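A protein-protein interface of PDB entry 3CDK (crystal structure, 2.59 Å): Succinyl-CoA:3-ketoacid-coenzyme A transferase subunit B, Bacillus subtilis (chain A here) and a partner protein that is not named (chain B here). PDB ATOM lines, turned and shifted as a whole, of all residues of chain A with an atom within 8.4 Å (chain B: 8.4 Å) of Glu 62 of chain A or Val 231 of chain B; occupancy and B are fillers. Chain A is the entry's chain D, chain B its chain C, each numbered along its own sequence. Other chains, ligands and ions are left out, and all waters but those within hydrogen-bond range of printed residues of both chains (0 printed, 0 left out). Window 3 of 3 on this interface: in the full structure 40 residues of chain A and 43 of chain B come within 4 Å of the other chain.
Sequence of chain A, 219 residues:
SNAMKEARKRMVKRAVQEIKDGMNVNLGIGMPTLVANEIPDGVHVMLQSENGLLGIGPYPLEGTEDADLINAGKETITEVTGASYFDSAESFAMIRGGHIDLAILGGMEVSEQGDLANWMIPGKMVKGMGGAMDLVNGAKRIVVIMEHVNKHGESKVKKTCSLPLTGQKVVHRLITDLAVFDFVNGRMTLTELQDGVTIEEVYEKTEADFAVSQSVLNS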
ATOM      1  N   PRO A  58      24.757 -18.514 -16.099  1.00  0.00           N
ATOM      2  CA  PRO A  58      24.580 -18.442 -14.645  1.00  0.00           C
ATOM      3  C   PRO A  58      25.281 -17.238 -14.022  1.00  0.00           C
ATOM      4  O   PRO A  58      26.012 -16.533 -14.705  1.00  0.00           O
ATOM      5  CB  PRO A  58      25.217 -19.749 -14.148  1.00  0.00           C
ATOM      6  CG  PRO A  58      25.328 -20.611 -15.349  1.00  0.00           C
ATOM      7  CD  PRO A  58      25.563 -19.688 -16.478  1.00  0.00           C
ATOM      8  N   TYR A  59      25.071 -17.030 -12.727  1.00  0.00           N
ATOM      9  CA  TYR A  59      25.684 -15.923 -12.003  1.00  0.00           C
ATOM     10  C   TYR A  59      27.210 -16.004 -11.906  1.00  0.00           C
ATOM     11  O   TYR A  59      27.754 -17.085 -11.775  1.00  0.00           O
ATOM     12  CB  TYR A  59      25.090 -15.850 -10.609  1.00  0.00           C
ATOM     13  CG  TYR A  59      23.608 -15.569 -10.595  1.00  0.00           C
ATOM     14  CD1 TYR A  59      23.070 -14.510 -11.328  1.00  0.00           C
ATOM     15  CD2 TYR A  59      22.749 -16.348  -9.818  1.00  0.00           C
ATOM     16  CE1 TYR A  59      21.715 -14.246 -11.306  1.00  0.00           C
ATOM     17  CE2 TYR A  59      21.403 -16.102  -9.780  1.00  0.00           C
ATOM     18  CZ  TYR A  59      20.888 -15.052 -10.525  1.00  0.00           C
ATOM     19  OH  TYR A  59      19.536 -14.811 -10.476  1.00  0.00           O
ATOM     20  N   PRO A  60      27.896 -14.843 -11.935  1.00  0.00           N
ATOM     21  CA  PRO A  60      29.355 -14.775 -12.023  1.00  0.00           C
ATOM     22  C   PRO A  60      30.055 -15.039 -10.708  1.00  0.00           C
ATOM     23  O   PRO A  60      29.485 -14.829  -9.638  1.00  0.00           O
ATOM     24  CB  PRO A  60      29.631 -13.326 -12.448  1.00  0.00           C
ATOM     25  CG  PRO A  60      28.339 -12.628 -12.451  1.00  0.00           C
ATOM     26  CD  PRO A  60      27.294 -13.503 -11.861  1.00  0.00           C
ATOM     27  N   LEU A  61      31.296 -15.492 -10.807  1.00  0.00           N
ATOM     28  CA  LEU A  61      32.155 -15.723  -9.669  1.00  0.00           C
ATOM     29  C   LEU A  61      32.505 -14.431  -8.953  1.00  0.00           C
ATOM     30  O   LEU A  61      32.876 -13.454  -9.599  1.00  0.00           O
ATOM     31  CB  LEU A  61      33.442 -16.358 -10.168  1.00  0.00           C
ATOM     32  CG  LEU A  61      33.799 -17.763  -9.673  1.00  0.00           C
ATOM     33  CD1 LEU A  61      34.394 -18.607 -10.834  1.00  0.00           C
ATOM     34  CD2 LEU A  61      34.756 -17.638  -8.495  1.00  0.00           C
ATOM     35  N   GLU A  62      32.408 -14.428  -7.624  1.00  0.00           N
ATOM     36  CA  GLU A  62      32.789 -13.259  -6.846  1.00  0.00           C
ATOM     37  C   GLU A  62      34.061 -12.608  -7.369  1.00  0.00           C
ATOM     38  O   GLU A  62      35.064 -13.281  -7.570  1.00  0.00           O
ATOM     39  CB  GLU A  62      32.972 -13.620  -5.374  1.00  0.00           C
ATOM     40  CG  GLU A  62      31.869 -13.075  -4.494  1.00  0.00           C
ATOM     41  CD  GLU A  62      31.994 -13.499  -3.044  1.00  0.00           C
ATOM     42  OE1 GLU A  62      32.734 -14.465  -2.755  1.00  0.00           O
ATOM     43  OE2 GLU A  62      31.339 -12.866  -2.189  1.00  0.00           O
ATOM     44  N   GLY A  63      34.017 -11.296  -7.584  1.00  0.00           N
ATOM     45  CA  GLY A  63      35.193 -10.553  -8.020  1.00  0.00           C
ATOM     46  C   GLY A  63      35.283 -10.506  -9.523  1.00  0.00           C
ATOM     47  O   GLY A  63      36.243  -9.967 -10.071  1.00  0.00           O
ATOM     48  N   THR A  64      34.264 -11.064 -10.179  1.00  0.00           N
ATOM     49  CA  THR A  64      34.212 -11.143 -11.625  1.00  0.00           C
ATOM     50  C   THR A  64      32.886 -10.702 -12.198  1.00  0.00           C
ATOM     51  O   THR A  64      32.677 -10.793 -13.416  1.00  0.00           O
ATOM     52  CB  THR A  64      34.499 -12.559 -12.124  1.00  0.00           C
ATOM     53  OG1 THR A  64      35.224 -12.468 -13.349  1.00  0.00           O
ATOM     54  CG2 THR A  64      33.208 -13.342 -12.379  1.00  0.00           C
ATOM     55  N   GLU A  65      31.979 -10.250 -11.340  1.00  0.00           N
ATOM     56  CA  GLU A  65      30.766  -9.603 -11.819  1.00  0.00           C
ATOM     57  C   GLU A  65      31.205  -8.435 -12.682  1.00  0.00           C
ATOM     58  O   GLU A  65      32.315  -7.916 -12.533  1.00  0.00           O
ATOM     59  CB  GLU A  65      29.902  -9.045 -10.675  1.00  0.00           C
ATOM     60  CG  GLU A  65      30.146  -9.650  -9.312  1.00  0.00           C
ATOM     61  CD  GLU A  65      31.305  -8.993  -8.574  1.00  0.00           C
ATOM     62  OE1 GLU A  65      32.427  -9.542  -8.590  1.00  0.00           O
ATOM     63  OE2 GLU A  65      31.092  -7.910  -7.985  1.00  0.00           O
ATOM     64  N   ASP A  66      30.325  -8.018 -13.578  1.00  0.00           N
ATOM     65  CA  ASP A  66      30.588  -6.878 -14.430  1.00  0.00           C
ATOM     66  C   ASP A  66      29.342  -5.990 -14.525  1.00  0.00           C
ATOM     67  O   ASP A  66      28.265  -6.442 -14.950  1.00  0.00           O
ATOM     68  CB  ASP A  66      31.045  -7.380 -15.802  1.00  0.00           C
ATOM     69  CG  ASP A  66      31.242  -6.263 -16.818  1.00  0.00           C
ATOM     70  OD1 ASP A  66      31.282  -5.068 -16.455  1.00  0.00           O
ATOM     71  OD2 ASP A  66      31.358  -6.606 -18.010  1.00  0.00           O
ATOM     72  N   GLU A  75      19.998  -8.020 -12.015  1.00  0.00           N
ATOM     73  CA  GLU A  75      21.000  -8.921 -11.451  1.00  0.00           C
ATOM     74  C   GLU A  75      22.208  -9.158 -12.357  1.00  0.00           C
ATOM     75  O   GLU A  75      22.092  -9.438 -13.545  1.00  0.00           O
ATOM     76  CB  GLU A  75      20.403 -10.281 -11.149  1.00  0.00           C
ATOM     77  CG  GLU A  75      19.168 -10.267 -10.338  1.00  0.00           C
ATOM     78  CD  GLU A  75      18.471 -11.595 -10.413  1.00  0.00           C
ATOM     79  OE1 GLU A  75      18.245 -12.066 -11.546  1.00  0.00           O
ATOM     80  OE2 GLU A  75      18.148 -12.162  -9.349  1.00  0.00           O
ATOM     81  N   THR A  76      23.370  -9.063 -11.746  1.00  0.00           N
ATOM     82  CA  THR A  76      24.643  -9.325 -12.372  1.00  0.00           C
ATOM     83  C   THR A  76      24.657 -10.792 -12.853  1.00  0.00           C
ATOM     84  O   THR A  76      24.249 -11.676 -12.111  1.00  0.00           O
ATOM     85  CB  THR A  76      25.747  -8.962 -11.313  1.00  0.00           C
ATOM     86  OG1 THR A  76      26.787  -8.186 -11.917  1.00  0.00           O
ATOM     87  CG2 THR A  76      26.298 -10.145 -10.592  1.00  0.00           C
ATOM     88  N   ILE A  77      25.059 -11.028 -14.105  1.00  0.00           N
ATOM     89  CA  ILE A  77      24.934 -12.355 -14.758  1.00  0.00           C
ATOM     90  C   ILE A  77      26.153 -12.755 -15.611  1.00  0.00           C
ATOM     91  O   ILE A  77      27.204 -12.122 -15.526  1.00  0.00           O
ATOM     92  CB  ILE A  77      23.637 -12.508 -15.666  1.00  0.00           C
ATOM     93  CG1 ILE A  77      23.536 -11.418 -16.721  1.00  0.00           C
ATOM     94  CG2 ILE A  77      22.341 -12.589 -14.845  1.00  0.00           C
ATOM     95  CD1 ILE A  77      22.896 -11.926 -17.991  1.00  0.00           C
ATOM     96  N   ILE B 226      26.086  -1.257  -9.627  1.00  0.00           N
ATOM     97  CA  ILE B 226      25.386  -2.519  -9.736  1.00  0.00           C
ATOM     98  C   ILE B 226      24.225  -2.551  -8.751  1.00  0.00           C
ATOM     99  O   ILE B 226      24.402  -2.333  -7.551  1.00  0.00           O
ATOM    100  CB  ILE B 226      26.332  -3.694  -9.445  1.00  0.00           C
ATOM    101  CG1 ILE B 226      27.619  -3.543 -10.262  1.00  0.00           C
ATOM    102  CG2 ILE B 226      25.631  -5.013  -9.726  1.00  0.00           C
ATOM    103  CD1 ILE B 226      28.588  -4.676 -10.106  1.00  0.00           C
ATOM    104  N   LYS B 228      21.871  -5.272  -8.343  1.00  0.00           N
ATOM    105  CA  LYS B 228      21.951  -6.568  -7.678  1.00  0.00           C
ATOM    106  C   LYS B 228      23.287  -7.268  -7.964  1.00  0.00           C
ATOM    107  O   LYS B 228      23.568  -7.636  -9.098  1.00  0.00           O
ATOM    108  CB  LYS B 228      20.761  -7.445  -8.074  1.00  0.00           C
ATOM    109  CG  LYS B 228      19.385  -6.776  -7.805  1.00  0.00           C
ATOM    110  CD  LYS B 228      18.281  -7.848  -7.816  1.00  0.00           C
ATOM    111  CE  LYS B 228      16.919  -7.237  -8.107  1.00  0.00           C
ATOM    112  NZ  LYS B 228      16.111  -8.104  -9.021  1.00  0.00           N
ATOM    113  N   ARG B 229      24.109  -7.421  -6.927  1.00  0.00           N
ATOM    114  CA  ARG B 229      25.353  -8.190  -7.014  1.00  0.00           C
ATOM    115  C   ARG B 229      25.111  -9.678  -6.758  1.00  0.00           C
ATOM    116  O   ARG B 229      25.378 -10.186  -5.636  1.00  0.00           O
ATOM    117  CB  ARG B 229      26.396  -7.646  -6.021  1.00  0.00           C
ATOM    118  CG  ARG B 229      27.372  -6.645  -6.622  1.00  0.00           C
ATOM    119  CD  ARG B 229      28.555  -6.350  -5.698  1.00  0.00           C
ATOM    120  NE  ARG B 229      29.717  -5.872  -6.449  1.00  0.00           N
ATOM    121  CZ  ARG B 229      29.914  -4.603  -6.818  1.00  0.00           C
ATOM    122  NH1 ARG B 229      29.031  -3.663  -6.508  1.00  0.00           N
ATOM    123  NH2 ARG B 229      30.998  -4.271  -7.507  1.00  0.00           N
ATOM    124  N   THR B 230      24.612 -10.376  -7.794  1.00  0.00           N
ATOM    125  CA  THR B 230      24.209 -11.775  -7.628  1.00  0.00           C
ATOM    126  C   THR B 230      25.282 -12.756  -8.105  1.00  0.00           C
ATOM    127  O   THR B 230      25.437 -12.979  -9.306  1.00  0.00           O
ATOM    128  CB  THR B 230      22.890 -12.056  -8.360  1.00  0.00           C
ATOM    129  OG1 THR B 230      21.997 -10.959  -8.152  1.00  0.00           O
ATOM    130  CG2 THR B 230      22.245 -13.318  -7.824  1.00  0.00           C
ATOM    131  N   VAL B 231      26.002 -13.348  -7.156  1.00  0.00           N
ATOM    132  CA  VAL B 231      27.214 -14.113  -7.454  1.00  0.00           C
ATOM    133  C   VAL B 231      27.148 -15.563  -6.973  1.00  0.00           C
ATOM    134  O   VAL B 231      26.637 -15.847  -5.891  1.00  0.00           O
ATOM    135  CB  VAL B 231      28.470 -13.443  -6.857  1.00  0.00           C
ATOM    136  CG1 VAL B 231      28.751 -12.132  -7.558  1.00  0.00           C
ATOM    137  CG2 VAL B 231      28.316 -13.231  -5.354  1.00  0.00           C
ATOM    138  N   GLN B 232      27.677 -16.471  -7.786  1.00  0.00           N
ATOM    139  CA  GLN B 232      27.732 -17.892  -7.439  1.00  0.00           C
ATOM    140  C   GLN B 232      28.917 -18.172  -6.521  1.00  0.00           C
ATOM    141  O   GLN B 232      29.241 -17.330  -5.650  1.00  0.00           O
ATOM    142  CB  GLN B 232      27.827 -18.762  -8.705  1.00  0.00           C
ATOM    143  CG  GLN B 232      26.491 -19.331  -9.216  1.00  0.00           C
ATOM    144  CD  GLN B 232      26.148 -20.707  -8.638  1.00  0.00           C
ATOM    145  OE1 GLN B 232      26.633 -21.085  -7.543  1.00  0.00           O
ATOM    146  NE2 GLN B 232      25.298 -21.457  -9.376  1.00  0.00           N
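The side-chain carboxylate (OE2) of Glu 75 of chain A is in hydrogen-bond range of the side-chain hydroxyl (OH) of Tyr 59 of chain A (3.2 Å). N of Gly 63 of chain A lies within hydrogen-bond range of OE1 of Glu 65 of chain A (2.6 Å).
Among the printed residues, merely in contact across the chains: Tyr 59 of chain A with Thr 230 of chain B (3.2 Å), Pro 60 of chain A with Thr 230 of chain B (3.2 Å), Pro 60 of chain A with Val 231 of chain B (3.2 Å), Glu 65 of chain A with Val 231 of chain B (3.3 Å), Glu 75 of chain A with Thr 230 of chain B (3.5 Å), Tyr 59 of chain A with Gln 232 of chain B (3.5 Å), Glu 75 of chain A with Lys 228 of chain B (3.6 Å) and Glu 62 of chain A with Val 231 of chain B (3.7 Å).
O of Lys 228 of chain B is in hydrogen-bond range of N of Thr 76 of chain A (3.0 Å). OE2 of Glu 65 of chain A is in salt-bridge range of NE of Arg 229 of chain B (2.9 Å). N of Gln 232 of chain B sits at hydrogen-bond distance from O of Pro 60 of chain A, at 3.1 Å. The backbone carbonyl oxygen (O) of Thr 76 of chain A sits close to the backbone carbonyl oxygen (O) of Thr 230 of chain B (3.3 Å).
Pro 58 of chain A touches none of the printed residues of chain B. Of the printed residues of chain B, Tyr 59 of chain A touches Thr 230 and Gln 232. Of the printed residues of chain B, Pro 60 of chain A touches Thr 230, Val 231 and Gln 232. Of the printed residues of chain B, Glu 75 of chain A touches Lys 228 (3.6 Å) and Thr 230 (3.5 Å). Of the printed residues of chain B, Thr 76 of chain A touches Lys 228 (3.0 Å) and Thr 230 (3.2 Å). Val 231 of chain B touches three residues of chain A. The nearest residue of chain A that does not touch Val 231 of chain B is Tyr 59 of chain A (4.2 Å). The nearest printed residue of chain B that does not touch Glu 75 of chain A is Arg 229 of chain B (5.7 Å).
Printed residues of chain B that touch a printed residue of chain A: Lys 228, Arg 229, Thr 230, Val 231 and Gln 232. Hydrophobic or aromatic side chains of chain B within 4 Å of the printed part of chain A: Val 231. Along chain B the printed residues that touch a printed residue of chain A span positions 228 to 232. Hydrophobic or aromatic side chains of chain A that line the printed part of chain B: Tyr 59 and Pro 60. Among the printed residues, 12 pairs touch across the chains.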
